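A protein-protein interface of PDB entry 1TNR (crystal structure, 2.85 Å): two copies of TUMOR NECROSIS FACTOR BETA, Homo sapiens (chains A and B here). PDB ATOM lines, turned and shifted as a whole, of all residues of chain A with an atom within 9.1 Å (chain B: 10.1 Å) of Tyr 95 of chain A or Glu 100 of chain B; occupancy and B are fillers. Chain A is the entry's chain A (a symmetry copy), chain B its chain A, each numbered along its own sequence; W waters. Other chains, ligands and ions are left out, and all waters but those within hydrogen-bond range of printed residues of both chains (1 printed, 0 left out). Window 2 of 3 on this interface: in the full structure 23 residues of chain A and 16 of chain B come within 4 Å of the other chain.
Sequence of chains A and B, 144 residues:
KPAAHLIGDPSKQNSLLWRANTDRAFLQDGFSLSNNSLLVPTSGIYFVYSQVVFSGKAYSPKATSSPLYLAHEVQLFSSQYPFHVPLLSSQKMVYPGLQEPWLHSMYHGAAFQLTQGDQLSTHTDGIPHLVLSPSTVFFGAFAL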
ATOM      1  N   ALA A  58      31.620  30.894  14.364  1.00  0.00           N
ATOM      2  CA  ALA A  58      32.155  29.604  14.820  1.00  0.00           C
ATOM      3  C   ALA A  58      33.367  29.202  13.966  1.00  0.00           C
ATOM      4  O   ALA A  58      33.238  29.019  12.737  1.00  0.00           O
ATOM      5  CB  ALA A  58      31.072  28.524  14.747  1.00  0.00           C
ATOM      6  N   ALA A  63      32.003  24.099  17.904  1.00  0.00           N
ATOM      7  CA  ALA A  63      31.123  25.258  18.102  1.00  0.00           C
ATOM      8  C   ALA A  63      29.804  25.230  17.301  1.00  0.00           C
ATOM      9  O   ALA A  63      28.852  25.921  17.646  1.00  0.00           O
ATOM     10  CB  ALA A  63      31.905  26.558  17.805  1.00  0.00           C
ATOM     11  N   THR A  64      29.742  24.409  16.263  1.00  0.00           N
ATOM     12  CA  THR A  64      28.560  24.303  15.412  1.00  0.00           C
ATOM     13  C   THR A  64      27.533  23.269  15.900  1.00  0.00           C
ATOM     14  O   THR A  64      26.395  23.222  15.409  1.00  0.00           O
ATOM     15  CB  THR A  64      29.018  23.978  13.974  1.00  0.00           C
ATOM     16  OG1 THR A  64      29.942  24.992  13.548  1.00  0.00           O
ATOM     17  CG2 THR A  64      27.845  23.907  13.001  1.00  0.00           C
ATOM     18  N   SER A  65      27.925  22.498  16.914  1.00  0.00           N
ATOM     19  CA  SER A  65      27.092  21.439  17.493  1.00  0.00           C
ATOM     20  C   SER A  65      25.872  21.960  18.254  1.00  0.00           C
ATOM     21  O   SER A  65      24.724  21.675  17.883  1.00  0.00           O
ATOM     22  CB  SER A  65      27.926  20.584  18.449  1.00  0.00           C
ATOM     23  OG  SER A  65      29.212  20.359  17.919  1.00  0.00           O
ATOM     24  N   SER A  66      26.143  22.665  19.358  1.00  0.00           N
ATOM     25  CA  SER A  66      25.100  23.236  20.214  1.00  0.00           C
ATOM     26  C   SER A  66      24.809  24.690  19.915  1.00  0.00           C
ATOM     27  O   SER A  66      25.703  25.459  19.540  1.00  0.00           O
ATOM     28  CB  SER A  66      25.459  23.100  21.703  1.00  0.00           C
ATOM     29  OG  SER A  66      25.144  21.802  22.200  1.00  0.00           O
ATOM     30  N   PRO A  67      23.537  25.079  20.070  1.00  0.00           N
ATOM     31  CA  PRO A  67      23.087  26.443  19.833  1.00  0.00           C
ATOM     32  C   PRO A  67      23.593  27.427  20.900  1.00  0.00           C
ATOM     33  O   PRO A  67      24.251  27.051  21.891  1.00  0.00           O
ATOM     34  CB  PRO A  67      21.566  26.299  19.878  1.00  0.00           C
ATOM     35  CG  PRO A  67      21.360  25.199  20.838  1.00  0.00           C
ATOM     36  CD  PRO A  67      22.391  24.213  20.392  1.00  0.00           C
ATOM     37  N   LEU A  68      23.298  28.699  20.656  1.00  0.00           N
ATOM     38  CA  LEU A  68      23.672  29.777  21.539  1.00  0.00           C
ATOM     39  C   LEU A  68      22.379  30.399  22.019  1.00  0.00           C
ATOM     40  O   LEU A  68      21.470  30.626  21.225  1.00  0.00           O
ATOM     41  CB  LEU A  68      24.443  30.813  20.749  1.00  0.00           C
ATOM     42  CG  LEU A  68      25.884  31.045  21.177  1.00  0.00           C
ATOM     43  CD1 LEU A  68      26.782  29.896  20.728  1.00  0.00           C
ATOM     44  CD2 LEU A  68      26.354  32.326  20.541  1.00  0.00           C
ATOM     45  N   TYR A  69      22.248  30.617  23.318  1.00  0.00           N
ATOM     46  CA  TYR A  69      21.036  31.254  23.839  1.00  0.00           C
ATOM     47  C   TYR A  69      21.364  32.745  24.048  1.00  0.00           C
ATOM     48  O   TYR A  69      22.371  33.059  24.682  1.00  0.00           O
ATOM     49  CB  TYR A  69      20.621  30.615  25.168  1.00  0.00           C
ATOM     50  CG  TYR A  69      19.491  31.339  25.868  1.00  0.00           C
ATOM     51  CD1 TYR A  69      18.182  31.282  25.377  1.00  0.00           C
ATOM     52  CD2 TYR A  69      19.729  32.076  27.025  1.00  0.00           C
ATOM     53  CE1 TYR A  69      17.140  31.943  26.024  1.00  0.00           C
ATOM     54  CE2 TYR A  69      18.704  32.738  27.677  1.00  0.00           C
ATOM     55  CZ  TYR A  69      17.411  32.671  27.173  1.00  0.00           C
ATOM     56  OH  TYR A  69      16.395  33.343  27.822  1.00  0.00           O
ATOM     57  N   LEU A  70      20.567  33.648  23.478  1.00  0.00           N
ATOM     58  CA  LEU A  70      20.813  35.080  23.640  1.00  0.00           C
ATOM     59  C   LEU A  70      19.577  35.697  24.266  1.00  0.00           C
ATOM     60  O   LEU A  70      18.448  35.416  23.835  1.00  0.00           O
ATOM     61  CB  LEU A  70      21.069  35.751  22.293  1.00  0.00           C
ATOM     62  CG  LEU A  70      22.135  35.171  21.374  1.00  0.00           C
ATOM     63  CD1 LEU A  70      22.004  35.781  19.982  1.00  0.00           C
ATOM     64  CD2 LEU A  70      23.491  35.406  21.957  1.00  0.00           C
ATOM     65  N   LYS A  92      16.340  34.698  21.882  1.00  0.00           N
ATOM     66  CA  LYS A  92      16.632  34.171  20.550  1.00  0.00           C
ATOM     67  C   LYS A  92      17.599  33.002  20.706  1.00  0.00           C
ATOM     68  O   LYS A  92      18.462  33.011  21.594  1.00  0.00           O
ATOM     69  CB  LYS A  92      17.313  35.266  19.711  1.00  0.00           C
ATOM     70  CG  LYS A  92      17.816  34.835  18.360  1.00  0.00           C
ATOM     71  CD  LYS A  92      16.639  34.488  17.472  1.00  0.00           C
ATOM     72  CE  LYS A  92      17.067  34.134  16.049  1.00  0.00           C
ATOM     73  NZ  LYS A  92      15.864  33.967  15.158  1.00  0.00           N
ATOM     74  N   MET A  93      17.441  31.982  19.872  1.00  0.00           N
ATOM     75  CA  MET A  93      18.349  30.840  19.906  1.00  0.00           C
ATOM     76  C   MET A  93      19.088  30.896  18.564  1.00  0.00           C
ATOM     77  O   MET A  93      18.467  31.050  17.511  1.00  0.00           O
ATOM     78  CB  MET A  93      17.567  29.538  20.031  1.00  0.00           C
ATOM     79  CG  MET A  93      18.394  28.395  20.571  1.00  0.00           C
ATOM     80  SD  MET A  93      18.606  28.441  22.343  1.00  0.00           S
ATOM     81  CE  MET A  93      17.351  27.366  22.798  1.00  0.00           C
ATOM     82  N   VAL A  94      20.410  30.826  18.595  1.00  0.00           N
ATOM     83  CA  VAL A  94      21.199  30.894  17.371  1.00  0.00           C
ATOM     84  C   VAL A  94      21.944  29.592  17.110  1.00  0.00           C
ATOM     85  O   VAL A  94      22.565  29.026  18.014  1.00  0.00           O
ATOM     86  CB  VAL A  94      22.189  32.105  17.436  1.00  0.00           C
ATOM     87  CG1 VAL A  94      23.428  31.847  16.646  1.00  0.00           C
ATOM     88  CG2 VAL A  94      21.517  33.347  16.889  1.00  0.00           C
ATOM     89  N   TYR A  95      21.856  29.117  15.871  1.00  0.00           N
ATOM     90  CA  TYR A  95      22.542  27.895  15.436  1.00  0.00           C
ATOM     91  C   TYR A  95      23.686  28.260  14.475  1.00  0.00           C
ATOM     92  O   TYR A  95      23.485  28.390  13.264  1.00  0.00           O
ATOM     93  CB  TYR A  95      21.550  26.946  14.767  1.00  0.00           C
ATOM     94  CG  TYR A  95      20.621  26.322  15.762  1.00  0.00           C
ATOM     95  CD1 TYR A  95      20.985  25.166  16.451  1.00  0.00           C
ATOM     96  CD2 TYR A  95      19.415  26.929  16.087  1.00  0.00           C
ATOM     97  CE1 TYR A  95      20.168  24.627  17.443  1.00  0.00           C
ATOM     98  CE2 TYR A  95      18.585  26.406  17.078  1.00  0.00           C
ATOM     99  CZ  TYR A  95      18.968  25.257  17.757  1.00  0.00           C
ATOM    100  OH  TYR A  95      18.148  24.735  18.735  1.00  0.00           O
ATOM    101  N   PRO A  96      24.893  28.467  15.017  1.00  0.00           N
ATOM    102  CA  PRO A  96      26.073  28.829  14.237  1.00  0.00           C
ATOM    103  C   PRO A  96      26.464  27.814  13.179  1.00  0.00           C
ATOM    104  O   PRO A  96      26.431  26.605  13.416  1.00  0.00           O
ATOM    105  CB  PRO A  96      27.159  28.934  15.305  1.00  0.00           C
ATOM    106  CG  PRO A  96      26.398  29.325  16.515  1.00  0.00           C
ATOM    107  CD  PRO A  96      25.240  28.379  16.439  1.00  0.00           C
ATOM    108  N   GLY A  97      26.798  28.337  12.003  1.00  0.00           N
ATOM    109  CA  GLY A  97      27.245  27.516  10.898  1.00  0.00           C
ATOM    110  C   GLY A  97      28.762  27.644  10.871  1.00  0.00           C
ATOM    111  O   GLY A  97      29.298  28.679  11.295  1.00  0.00           O
ATOM    112  N   LEU A  98      29.464  26.619  10.380  1.00  0.00           N
ATOM    113  CA  LEU A  98      30.930  26.652  10.346  1.00  0.00           C
ATOM    114  C   LEU A  98      31.484  27.751   9.448  1.00  0.00           C
ATOM    115  O   LEU A  98      31.310  27.701   8.228  1.00  0.00           O
ATOM    116  CB  LEU A  98      31.507  25.296   9.917  1.00  0.00           C
ATOM    117  CG  LEU A  98      33.041  25.192   9.821  1.00  0.00           C
ATOM    118  CD1 LEU A  98      33.709  25.246  11.202  1.00  0.00           C
ATOM    119  CD2 LEU A  98      33.394  23.904   9.113  1.00  0.00           C
ATOM    120  N   GLU A 100      30.564  30.858   8.925  1.00  0.00           N
ATOM    121  CA  GLU A 100      29.609  31.887   8.497  1.00  0.00           C
ATOM    122  C   GLU A 100      29.263  32.732   9.713  1.00  0.00           C
ATOM    123  O   GLU A 100      28.702  32.219  10.681  1.00  0.00           O
ATOM    124  CB  GLU A 100      28.320  31.238   8.001  1.00  0.00           C
ATOM    125  CG  GLU A 100      28.486  30.107   6.998  1.00  0.00           C
ATOM    126  CD  GLU A 100      27.288  29.157   6.981  1.00  0.00           C
ATOM    127  OE1 GLU A 100      26.740  28.834   8.059  1.00  0.00           O
ATOM    128  OE2 GLU A 100      26.897  28.719   5.885  1.00  0.00           O
ATOM    129  N   PRO A 101      29.562  34.043   9.672  1.00  0.00           N
ATOM    130  CA  PRO A 101      29.252  34.898  10.820  1.00  0.00           C
ATOM    131  C   PRO A 101      27.745  35.183  10.921  1.00  0.00           C
ATOM    132  O   PRO A 101      27.052  35.301   9.903  1.00  0.00           O
ATOM    133  CB  PRO A 101      30.045  36.171  10.514  1.00  0.00           C
ATOM    134  CG  PRO A 101      29.911  36.285   9.049  1.00  0.00           C
ATOM    135  CD  PRO A 101      30.123  34.841   8.566  1.00  0.00           C
ATOM    136  N   TRP A 102      27.237  35.274  12.147  1.00  0.00           N
ATOM    137  CA  TRP A 102      25.825  35.557  12.360  1.00  0.00           C
ATOM    138  C   TRP A 102      25.662  36.917  13.049  1.00  0.00           C
ATOM    139  O   TRP A 102      26.554  37.353  13.792  1.00  0.00           O
ATOM    140  CB  TRP A 102      25.196  34.441  13.169  1.00  0.00           C
ATOM    141  CG  TRP A 102      25.923  34.136  14.406  1.00  0.00           C
ATOM    142  CD1 TRP A 102      26.916  33.227  14.568  1.00  0.00           C
ATOM    143  CD2 TRP A 102      25.699  34.726  15.684  1.00  0.00           C
ATOM    144  NE1 TRP A 102      27.337  33.209  15.877  1.00  0.00           N
ATOM    145  CE2 TRP A 102      26.615  34.133  16.583  1.00  0.00           C
ATOM    146  CE3 TRP A 102      24.829  35.726  16.156  1.00  0.00           C
ATOM    147  CZ2 TRP A 102      26.665  34.475  17.929  1.00  0.00           C
ATOM    148  CZ3 TRP A 102      24.878  36.069  17.499  1.00  0.00           C
ATOM    149  CH2 TRP A 102      25.800  35.456  18.368  1.00  0.00           C
ATOM    150  N   SER B  55       8.157  30.191  20.354  1.00  0.00           N
ATOM    151  CA  SER B  55       9.099  29.083  20.505  1.00  0.00           C
ATOM    152  C   SER B  55       8.497  27.783  19.953  1.00  0.00           C
ATOM    153  O   SER B  55       7.303  27.700  19.687  1.00  0.00           O
ATOM    154  CB  SER B  55       9.425  28.892  21.972  1.00  0.00           C
ATOM    155  OG  SER B  55       8.262  28.425  22.626  1.00  0.00           O
ATOM    156  N   GLY B  56       9.329  26.769  19.772  1.00  0.00           N
ATOM    157  CA  GLY B  56       8.848  25.487  19.290  1.00  0.00           C
ATOM    158  C   GLY B  56       9.977  24.481  19.234  1.00  0.00           C
ATOM    159  O   GLY B  56      11.125  24.821  19.491  1.00  0.00           O
ATOM    160  N   LYS B  57       9.652  23.236  18.910  1.00  0.00           N
ATOM    161  CA  LYS B  57      10.655  22.177  18.781  1.00  0.00           C
ATOM    162  C   LYS B  57      10.029  21.029  17.988  1.00  0.00           C
ATOM    163  O   LYS B  57       9.202  20.295  18.528  1.00  0.00           O
ATOM    164  CB  LYS B  57      11.105  21.694  20.167  1.00  0.00           C
ATOM    165  CG  LYS B  57      12.211  20.661  20.160  1.00  0.00           C
ATOM    166  CD  LYS B  57      12.426  20.149  21.561  1.00  0.00           C
ATOM    167  CE  LYS B  57      12.897  18.722  21.527  1.00  0.00           C
ATOM    168  NZ  LYS B  57      13.026  18.136  22.881  1.00  0.00           N
ATOM    169  N   ALA B  58      10.389  20.914  16.706  1.00  0.00           N
ATOM    170  CA  ALA B  58       9.887  19.871  15.801  1.00  0.00           C
ATOM    171  C   ALA B  58      10.339  18.486  16.288  1.00  0.00           C
ATOM    172  O   ALA B  58      11.555  18.212  16.363  1.00  0.00           O
ATOM    173  CB  ALA B  58      10.382  20.121  14.374  1.00  0.00           C
ATOM    174  N   TYR B  59       9.357  17.641  16.641  1.00  0.00           N
ATOM    175  CA  TYR B  59       9.598  16.283  17.149  1.00  0.00           C
ATOM    176  C   TYR B  59       9.734  15.215  16.083  1.00  0.00           C
ATOM    177  O   TYR B  59      10.403  14.207  16.301  1.00  0.00           O
ATOM    178  CB  TYR B  59       8.501  15.864  18.141  1.00  0.00           C
ATOM    179  CG  TYR B  59       8.829  16.242  19.569  1.00  0.00           C
ATOM    180  CD1 TYR B  59       8.557  17.525  20.056  1.00  0.00           C
ATOM    181  CD2 TYR B  59       9.457  15.331  20.424  1.00  0.00           C
ATOM    182  N   SER B  60       9.142  15.468  14.919  1.00  0.00           N
ATOM    183  CA  SER B  60       9.155  14.512  13.820  1.00  0.00           C
ATOM    184  C   SER B  60       9.680  15.135  12.535  1.00  0.00           C
ATOM    185  O   SER B  60       9.622  16.349  12.366  1.00  0.00           O
ATOM    186  CB  SER B  60       7.730  14.003  13.588  1.00  0.00           C
ATOM    187  OG  SER B  60       6.866  15.082  13.258  1.00  0.00           O
ATOM    188  N   ALA B  63       7.441  17.625  10.433  1.00  0.00           N
ATOM    189  CA  ALA B  63       7.446  19.018  10.898  1.00  0.00           C
ATOM    190  C   ALA B  63       8.623  19.878  10.396  1.00  0.00           C
ATOM    191  O   ALA B  63       8.548  21.102  10.401  1.00  0.00           O
ATOM    192  CB  ALA B  63       7.377  19.048  12.443  1.00  0.00           C
ATOM    193  N   THR B  64       9.687  19.238   9.931  1.00  0.00           N
ATOM    194  CA  THR B  64      10.875  19.934   9.446  1.00  0.00           C
ATOM    195  C   THR B  64      10.819  20.291   7.952  1.00  0.00           C
ATOM    196  O   THR B  64      11.649  21.065   7.451  1.00  0.00           O
ATOM    197  CB  THR B  64      12.113  19.064   9.752  1.00  0.00           C
ATOM    198  OG1 THR B  64      12.144  18.793  11.162  1.00  0.00           O
ATOM    199  CG2 THR B  64      13.411  19.746   9.328  1.00  0.00           C
ATOM    200  N   VAL B  94       9.961  30.798   9.945  1.00  0.00           N
ATOM    201  CA  VAL B  94      10.862  29.930  10.693  1.00  0.00           C
ATOM    202  C   VAL B  94      10.970  28.551  10.056  1.00  0.00           C
ATOM    203  O   VAL B  94       9.963  27.943   9.689  1.00  0.00           O
ATOM    204  CB  VAL B  94      10.393  29.825  12.183  1.00  0.00           C
ATOM    205  CG1 VAL B  94      10.766  28.513  12.788  1.00  0.00           C
ATOM    206  CG2 VAL B  94      11.029  30.931  13.000  1.00  0.00           C
ATOM    207  N   TYR B  95      12.206  28.079   9.913  1.00  0.00           N
ATOM    208  CA  TYR B  95      12.492  26.753   9.354  1.00  0.00           C
ATOM    209  C   TYR B  95      13.009  25.825  10.466  1.00  0.00           C
ATOM    210  O   TYR B  95      14.207  25.786  10.760  1.00  0.00           O
ATOM    211  CB  TYR B  95      13.513  26.869   8.223  1.00  0.00           C
ATOM    212  CG  TYR B  95      12.915  27.489   6.998  1.00  0.00           C
ATOM    213  CD1 TYR B  95      12.236  26.709   6.062  1.00  0.00           C
ATOM    214  CD2 TYR B  95      12.945  28.865   6.811  1.00  0.00           C
ATOM    215  CE1 TYR B  95      11.600  27.287   4.965  1.00  0.00           C
ATOM    216  CE2 TYR B  95      12.313  29.461   5.719  1.00  0.00           C
ATOM    217  CZ  TYR B  95      11.637  28.668   4.802  1.00  0.00           C
ATOM    218  OH  TYR B  95      11.014  29.253   3.720  1.00  0.00           O
ATOM    219  N   PRO B  96      12.097  25.095  11.122  1.00  0.00           N
ATOM    220  CA  PRO B  96      12.431  24.177  12.207  1.00  0.00           C
ATOM    221  C   PRO B  96      13.384  23.063  11.818  1.00  0.00           C
ATOM    222  O   PRO B  96      13.263  22.470  10.744  1.00  0.00           O
ATOM    223  CB  PRO B  96      11.068  23.606  12.592  1.00  0.00           C
ATOM    224  CG  PRO B  96      10.137  24.704  12.240  1.00  0.00           C
ATOM    225  CD  PRO B  96      10.650  25.088  10.887  1.00  0.00           C
ATOM    226  N   GLY B  97      14.349  22.822  12.700  1.00  0.00           N
ATOM    227  CA  GLY B  97      15.314  21.760  12.510  1.00  0.00           C
ATOM    228  C   GLY B  97      14.847  20.611  13.394  1.00  0.00           C
ATOM    229  O   GLY B  97      14.197  20.852  14.422  1.00  0.00           O
ATOM    230  N   LEU B  98      15.166  19.369  13.019  1.00  0.00           N
ATOM    231  CA  LEU B  98      14.729  18.207  13.800  1.00  0.00           C
ATOM    232  C   LEU B  98      15.318  18.172  15.205  1.00  0.00           C
ATOM    233  O   LEU B  98      16.530  18.010  15.365  1.00  0.00           O
ATOM    234  CB  LEU B  98      15.055  16.894  13.073  1.00  0.00           C
ATOM    235  CG  LEU B  98      14.666  15.588  13.789  1.00  0.00           C
ATOM    236  CD1 LEU B  98      13.144  15.393  13.845  1.00  0.00           C
ATOM    237  CD2 LEU B  98      15.321  14.430  13.070  1.00  0.00           C
ATOM    238  N   GLN B  99      14.448  18.354  16.201  1.00  0.00           N
ATOM    239  CA  GLN B  99      14.796  18.324  17.631  1.00  0.00           C
ATOM    240  C   GLN B  99      15.443  19.562  18.260  1.00  0.00           C
ATOM    241  O   GLN B  99      15.544  19.640  19.486  1.00  0.00           O
ATOM    242  CB  GLN B  99      15.634  17.086  17.968  1.00  0.00           C
ATOM    243  CG  GLN B  99      15.190  16.385  19.244  1.00  0.00           C
ATOM    244  CD  GLN B  99      13.753  15.868  19.174  1.00  0.00           C
ATOM    245  OE1 GLN B  99      12.965  16.064  20.107  1.00  0.00           O
ATOM    246  NE2 GLN B  99      13.415  15.179  18.077  1.00  0.00           N
ATOM    247  N   GLU B 100      15.868  20.519  17.433  1.00  0.00           N
ATOM    248  CA  GLU B 100      16.498  21.760  17.901  1.00  0.00           C
ATOM    249  C   GLU B 100      15.393  22.778  18.135  1.00  0.00           C
ATOM    250  O   GLU B 100      14.696  23.160  17.195  1.00  0.00           O
ATOM    251  CB  GLU B 100      17.425  22.319  16.826  1.00  0.00           C
ATOM    252  CG  GLU B 100      18.407  21.332  16.214  1.00  0.00           C
ATOM    253  CD  GLU B 100      18.877  21.759  14.823  1.00  0.00           C
ATOM    254  OE1 GLU B 100      18.057  22.260  14.020  1.00  0.00           O
ATOM    255  OE2 GLU B 100      20.070  21.582  14.522  1.00  0.00           O
ATOM    256  N   PRO B 101      15.237  23.259  19.382  1.00  0.00           N
ATOM    257  CA  PRO B 101      14.186  24.241  19.659  1.00  0.00           C
ATOM    258  C   PRO B 101      14.547  25.628  19.105  1.00  0.00           C
ATOM    259  O   PRO B 101      15.721  26.019  19.092  1.00  0.00           O
ATOM    260  CB  PRO B 101      14.125  24.244  21.189  1.00  0.00           C
ATOM    261  CG  PRO B 101      15.544  24.087  21.563  1.00  0.00           C
ATOM    262  CD  PRO B 101      16.044  23.006  20.591  1.00  0.00           C
ATOM    263  N   TRP B 102      13.544  26.360  18.630  1.00  0.00           N
ATOM    264  CA  TRP B 102      13.769  27.695  18.096  1.00  0.00           C
ATOM    265  C   TRP B 102      13.067  28.736  18.975  1.00  0.00           C
ATOM    266  O   TRP B 102      12.048  28.431  19.612  1.00  0.00           O
ATOM    267  CB  TRP B 102      13.291  27.759  16.660  1.00  0.00           C
ATOM    268  CG  TRP B 102      11.914  27.286  16.483  1.00  0.00           C
ATOM    269  CD1 TRP B 102      11.514  26.022  16.197  1.00  0.00           C
ATOM    270  CD2 TRP B 102      10.733  28.080  16.554  1.00  0.00           C
ATOM    271  NE1 TRP B 102      10.145  25.969  16.084  1.00  0.00           N
ATOM    272  CE2 TRP B 102       9.637  27.219  16.314  1.00  0.00           C
ATOM    273  CE3 TRP B 102      10.487  29.437  16.827  1.00  0.00           C
ATOM    274  CZ2 TRP B 102       8.323  27.671  16.303  1.00  0.00           C
ATOM    275  CZ3 TRP B 102       9.175  29.891  16.816  1.00  0.00           C
ATOM    276  CH2 TRP B 102       8.108  29.007  16.571  1.00  0.00           C
ATOM    277  N   LEU B 103      13.612  29.952  18.993  1.00  0.00           N
ATOM    278  CA  LEU B 103      13.108  31.058  19.805  1.00  0.00           C
ATOM    279  C   LEU B 103      13.227  32.368  19.034  1.00  0.00           C
ATOM    280  O   LEU B 103      14.329  32.740  18.608  1.00  0.00           O
ATOM    281  CB  LEU B 103      13.972  31.196  21.056  1.00  0.00           C
ATOM    282  CG  LEU B 103      13.430  30.911  22.438  1.00  0.00           C
ATOM    283  CD1 LEU B 103      14.509  31.247  23.436  1.00  0.00           C
ATOM    284  CD2 LEU B 103      12.231  31.767  22.679  1.00  0.00           C
ATOM    285  N   HIS B 104      12.129  33.107  18.920  1.00  0.00           N
ATOM    286  CA  HIS B 104      12.151  34.382  18.219  1.00  0.00           C
ATOM    287  C   HIS B 104      11.365  35.484  18.920  1.00  0.00           C
ATOM    288  O   HIS B 104      10.321  35.224  19.520  1.00  0.00           O
ATOM    289  CB  HIS B 104      11.576  34.224  16.832  1.00  0.00           C
ATOM    290  CG  HIS B 104      11.812  35.423  15.973  1.00  0.00           C
ATOM    291  ND1 HIS B 104      13.087  35.893  15.705  1.00  0.00           N
ATOM    292  CD2 HIS B 104      10.957  36.270  15.359  1.00  0.00           C
ATOM    293  CE1 HIS B 104      12.996  36.981  14.958  1.00  0.00           C
ATOM    294  NE2 HIS B 104      11.717  37.232  14.734  1.00  0.00           N
HETATM  295  O   HOH W   1      15.843  30.197  17.198  1.00  0.00           O
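Tyr 95 of chain A touches Glu 100 of chain B, but with the chains exchanged Glu 100 of chain A does not touch Tyr 95 of chain B (13.2 Å). Tyr 95 of chain A touches Pro 101 of chain B, but with the chains exchanged Pro 101 of chain A does not touch Tyr 95 of chain B (15.8 Å). 11 positions are printed for both chains. Of the 7 pairs that touch across the chains among the printed residues, none has its exchanged pair printed and touching as well.
Water W1 bridges O of Met 93 of chain A (2.8 Å) and N of Leu 103 of chain B (2.9 Å).
A ring nitrogen (ND1) of His 104 of chain B sits at hydrogen-bond distance from the side-chain amino group of Lys 92 of chain A. OH of Tyr 95 of chain A lies within hydrogen-bond range of O of Pro 101 of chain B, at 2.8 Å. The backbone NH (N) of Met 93 of chain A is in hydrogen-bond range of the backbone carbonyl oxygen (O) of Leu 103 of chain B (3.4 Å).
Tyr 95 of chain A touches two residues of chain B. No residue of chain B comes within 4 Å of Val 94 of chain A. No residue of chain B comes within 4 Å of Pro 96 of chain A. Gly 97 of chain B touches none of the printed residues of chain A. Of chain A, only Met 93 and Tyr 95 come within 4 Å of Pro 101 of chain B. Of the printed residues of chain B, Lys 92 of chain A touches Leu 103 (3.1 Å) and His 104 (3.4 Å). Of the printed residues of chain A, Leu 103 of chain B touches Tyr 69, Lys 92 and Met 93. Pro 101 of chain A touches none of the printed residues of chain B. Ala 58 of chain B touches none of the printed residues of chain A. The nearest residue of chain B that does not touch Tyr 95 of chain A is Trp 102 of chain B (4.9 Å). The nearest residue of chain A that does not touch Glu 100 of chain B is Ser 65 of chain A (5.7 Å).
Among the printed residues, merely in contact across the chains: Tyr 69 of chain A with Leu 103 of chain B (3.8 Å), Lys 92 of chain A with Leu 103 of chain B (3.1 Å), Met 93 of chain A with Pro 101 of chain B (3.9 Å) and Tyr 95 of chain A with Glu 100 of chain B (3.2 Å).
Of the 19 printed residues of chain B, 4 touch a printed residue of chain A. Hydrophobic or aromatic side chains of chain B within 4 Å of the printed part of chain A: Pro 101, Leu 103 and His 104. Along chain B the printed residues that touch a printed residue of chain A span positions 100 to 104. Of the 19 printed residues of chain A, 4 touch a printed residue of chain B. Hydrophobic or aromatic side chains of chain A within 4 Å of the printed part of chain B: Tyr 69, Met 93 and Tyr 95. Along chain A the printed residues that touch a printed residue of chain B span positions 69 to 95. Among the printed residues, 7 pairs touch across the chains.
The backbone carbonyl oxygen (O) of Lys 92 of chain A is in hydrogen-bond range of the backbone NH (N) of Leu 70 of chain A (2.9 Å).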
